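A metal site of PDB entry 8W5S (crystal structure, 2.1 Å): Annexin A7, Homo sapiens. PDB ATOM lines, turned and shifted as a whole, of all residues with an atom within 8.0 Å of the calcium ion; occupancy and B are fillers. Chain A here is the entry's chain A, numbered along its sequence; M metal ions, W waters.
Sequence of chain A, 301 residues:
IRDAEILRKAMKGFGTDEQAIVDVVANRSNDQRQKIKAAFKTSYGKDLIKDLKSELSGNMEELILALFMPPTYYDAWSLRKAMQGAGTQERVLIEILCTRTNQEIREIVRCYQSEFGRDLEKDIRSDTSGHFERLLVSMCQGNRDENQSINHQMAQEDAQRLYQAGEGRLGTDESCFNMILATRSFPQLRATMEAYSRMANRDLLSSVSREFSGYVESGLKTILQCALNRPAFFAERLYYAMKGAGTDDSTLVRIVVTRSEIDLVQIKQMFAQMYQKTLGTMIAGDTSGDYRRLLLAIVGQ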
ATOM      1  N   ARG A   8       3.440  26.889   8.958  1.00  0.00           N
ATOM      2  CA  ARG A   8       2.654  26.974   7.730  1.00  0.00           C
ATOM      3  C   ARG A   8       3.385  27.801   6.674  1.00  0.00           C
ATOM      4  O   ARG A   8       3.435  27.415   5.502  1.00  0.00           O
ATOM      5  CB  ARG A   8       1.284  27.582   8.039  1.00  0.00           C
ATOM      6  CG  ARG A   8       0.590  28.175   6.827  1.00  0.00           C
ATOM      7  CD  ARG A   8      -0.105  27.105   6.017  1.00  0.00           C
ATOM      8  NE  ARG A   8      -1.359  27.585   5.449  1.00  0.00           N
ATOM      9  CZ  ARG A   8      -1.894  27.126   4.330  1.00  0.00           C
ATOM     10  NH1 ARG A   8      -1.311  26.163   3.625  1.00  0.00           N
ATOM     11  NH2 ARG A   8      -3.040  27.647   3.889  1.00  0.00           N
ATOM     12  N   LYS A   9       3.971  28.926   7.086  1.00  0.00           N
ATOM     13  CA  LYS A   9       4.746  29.734   6.155  1.00  0.00           C
ATOM     14  C   LYS A   9       5.970  28.985   5.662  1.00  0.00           C
ATOM     15  O   LYS A   9       6.292  29.021   4.467  1.00  0.00           O
ATOM     16  CB  LYS A   9       5.173  31.047   6.833  1.00  0.00           C
ATOM     17  CG  LYS A   9       4.864  32.299   6.035  1.00  0.00           C
ATOM     18  CD  LYS A   9       5.189  33.541   6.857  1.00  0.00           C
ATOM     19  CE  LYS A   9       6.692  33.797   6.907  1.00  0.00           C
ATOM     20  NZ  LYS A   9       7.015  35.245   6.881  1.00  0.00           N
ATOM     21  N   ALA A  10       6.672  28.288   6.555  1.00  0.00           N
ATOM     22  CA  ALA A  10       7.897  27.595   6.191  1.00  0.00           C
ATOM     23  C   ALA A  10       7.626  26.348   5.355  1.00  0.00           C
ATOM     24  O   ALA A  10       8.544  25.865   4.681  1.00  0.00           O
ATOM     25  CB  ALA A  10       8.686  27.217   7.444  1.00  0.00           C
ATOM     26  N   MET A  11       6.401  25.819   5.373  1.00  0.00           N
ATOM     27  CA  MET A  11       6.037  24.712   4.492  1.00  0.00           C
ATOM     28  C   MET A  11       5.351  25.155   3.220  1.00  0.00           C
ATOM     29  O   MET A  11       5.302  24.373   2.257  1.00  0.00           O
ATOM     30  CB  MET A  11       5.116  23.727   5.220  1.00  0.00           C
ATOM     31  CG  MET A  11       5.794  22.892   6.299  1.00  0.00           C
ATOM     32  SD  MET A  11       4.634  21.798   7.135  1.00  0.00           S
ATOM     33  CE  MET A  11       3.732  22.961   8.164  1.00  0.00           C
ATOM     34  N   LYS A  12       4.830  26.375   3.173  1.00  0.00           N
ATOM     35  CA  LYS A  12       4.091  26.830   2.003  1.00  0.00           C
ATOM     36  C   LYS A  12       5.031  27.006   0.807  1.00  0.00           C
ATOM     37  O   LYS A  12       6.223  27.272   0.956  1.00  0.00           O
ATOM     38  CB  LYS A  12       3.369  28.143   2.291  1.00  0.00           C
ATOM     39  CG  LYS A  12       1.890  28.148   1.898  1.00  0.00           C
ATOM     40  CD  LYS A  12       1.380  26.744   1.566  1.00  0.00           C
ATOM     41  CE  LYS A  12       1.081  26.597   0.080  1.00  0.00           C
ATOM     42  NZ  LYS A  12       1.813  25.446  -0.521  1.00  0.00           N
ATOM     43  N   GLY A  13       4.466  26.846  -0.385  1.00  0.00           N
ATOM     44  CA  GLY A  13       5.221  26.976  -1.605  1.00  0.00           C
ATOM     45  C   GLY A  13       6.130  25.778  -1.858  1.00  0.00           C
ATOM     46  O   GLY A  13       6.220  24.831  -1.074  1.00  0.00           O
ATOM     47  N   PHE A  14       6.794  25.840  -3.008  1.00  0.00           N
ATOM     48  CA  PHE A  14       7.772  24.825  -3.371  1.00  0.00           C
ATOM     49  C   PHE A  14       8.846  24.699  -2.294  1.00  0.00           C
ATOM     50  O   PHE A  14       9.346  25.712  -1.775  1.00  0.00           O
ATOM     51  CB  PHE A  14       8.413  25.186  -4.714  1.00  0.00           C
ATOM     52  CG  PHE A  14       9.453  24.204  -5.192  1.00  0.00           C
ATOM     53  CD1 PHE A  14       9.071  23.001  -5.759  1.00  0.00           C
ATOM     54  CD2 PHE A  14      10.801  24.489  -5.073  1.00  0.00           C
ATOM     55  CE1 PHE A  14      10.024  22.091  -6.199  1.00  0.00           C
ATOM     56  CE2 PHE A  14      11.757  23.586  -5.506  1.00  0.00           C
ATOM     57  CZ  PHE A  14      11.362  22.392  -6.064  1.00  0.00           C
ATOM     58  N   GLY A  15       9.190  23.465  -1.950  1.00  0.00           N
ATOM     59  CA  GLY A  15      10.228  23.224  -0.979  1.00  0.00           C
ATOM     60  C   GLY A  15       9.765  23.421   0.451  1.00  0.00           C
ATOM     61  O   GLY A  15       8.566  23.523   0.765  1.00  0.00           O
ATOM     62  N   THR A  16      10.751  23.476   1.343  1.00  0.00           N
ATOM     63  CA  THR A  16      10.551  23.663   2.774  1.00  0.00           C
ATOM     64  C   THR A  16      11.667  24.553   3.315  1.00  0.00           C
ATOM     65  O   THR A  16      12.821  24.398   2.918  1.00  0.00           O
ATOM     66  CB  THR A  16      10.558  22.331   3.532  1.00  0.00           C
ATOM     67  OG1 THR A  16       9.739  21.369   2.861  1.00  0.00           O
ATOM     68  CG2 THR A  16      10.052  22.523   4.966  1.00  0.00           C
ATOM     69  N   ASP A  51       0.926  17.474   7.682  1.00  0.00           N
ATOM     70  CA  ASP A  51       1.601  18.425   6.803  1.00  0.00           C
ATOM     71  C   ASP A  51       3.118  18.365   6.987  1.00  0.00           C
ATOM     72  O   ASP A  51       3.857  18.582   6.027  1.00  0.00           O
ATOM     73  CB  ASP A  51       1.089  19.833   7.077  1.00  0.00           C
ATOM     74  CG  ASP A  51      -0.107  20.194   6.225  1.00  0.00           C
ATOM     75  OD1 ASP A  51      -0.415  19.438   5.273  1.00  0.00           O
ATOM     76  OD2 ASP A  51      -0.760  21.218   6.511  1.00  0.00           O
ATOM     77  N   SER A  54       4.487  15.349   5.119  1.00  0.00           N
ATOM     78  CA  SER A  54       4.515  15.497   3.671  1.00  0.00           C
ATOM     79  C   SER A  54       5.696  16.316   3.196  1.00  0.00           C
ATOM     80  O   SER A  54       6.167  16.116   2.068  1.00  0.00           O
ATOM     81  CB  SER A  54       3.209  16.142   3.193  1.00  0.00           C
ATOM     82  OG  SER A  54       2.905  17.296   3.953  1.00  0.00           O
ATOM     83  N   GLU A  55       6.205  17.231   4.022  1.00  0.00           N
ATOM     84  CA  GLU A  55       7.257  18.154   3.610  1.00  0.00           C
ATOM     85  C   GLU A  55       8.593  17.898   4.311  1.00  0.00           C
ATOM     86  O   GLU A  55       9.567  18.593   4.020  1.00  0.00           O
ATOM     87  CB  GLU A  55       6.808  19.601   3.830  1.00  0.00           C
ATOM     88  CG  GLU A  55       6.001  20.164   2.679  1.00  0.00           C
ATOM     89  CD  GLU A  55       6.473  21.540   2.244  1.00  0.00           C
ATOM     90  OE1 GLU A  55       7.208  22.173   3.018  1.00  0.00           O
ATOM     91  OE2 GLU A  55       6.109  21.964   1.130  1.00  0.00           O
HETATM   92 CA    CA M   1       4.780  23.025  -0.240  1.00  0.00          CA
HETATM   93  O   HOH W   1       7.691  21.582  -1.179  1.00  0.00           O
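The side-chain carboxylate (OE1) of Glu 55 is in hydrogen-bond range of the side-chain hydroxyl (OG1) of Thr 16 (2.7 Å).
Merely in contact with the calcium ion: Lys 12 and Gly 15. Of the 12 residues printed, 5 come within 4 Å of the calcium ion. The nearest printed residue that does not touch the calcium ion is Phe 14 (4.4 Å).
The calcium ion is bound by OE2 of Glu 55 (2.2 Å). O of Gly 13 binds the calcium ion. The calcium ion is bound by O of Met 11, 2.9 Å away. The calcium ion has three donor atoms within binding distance.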
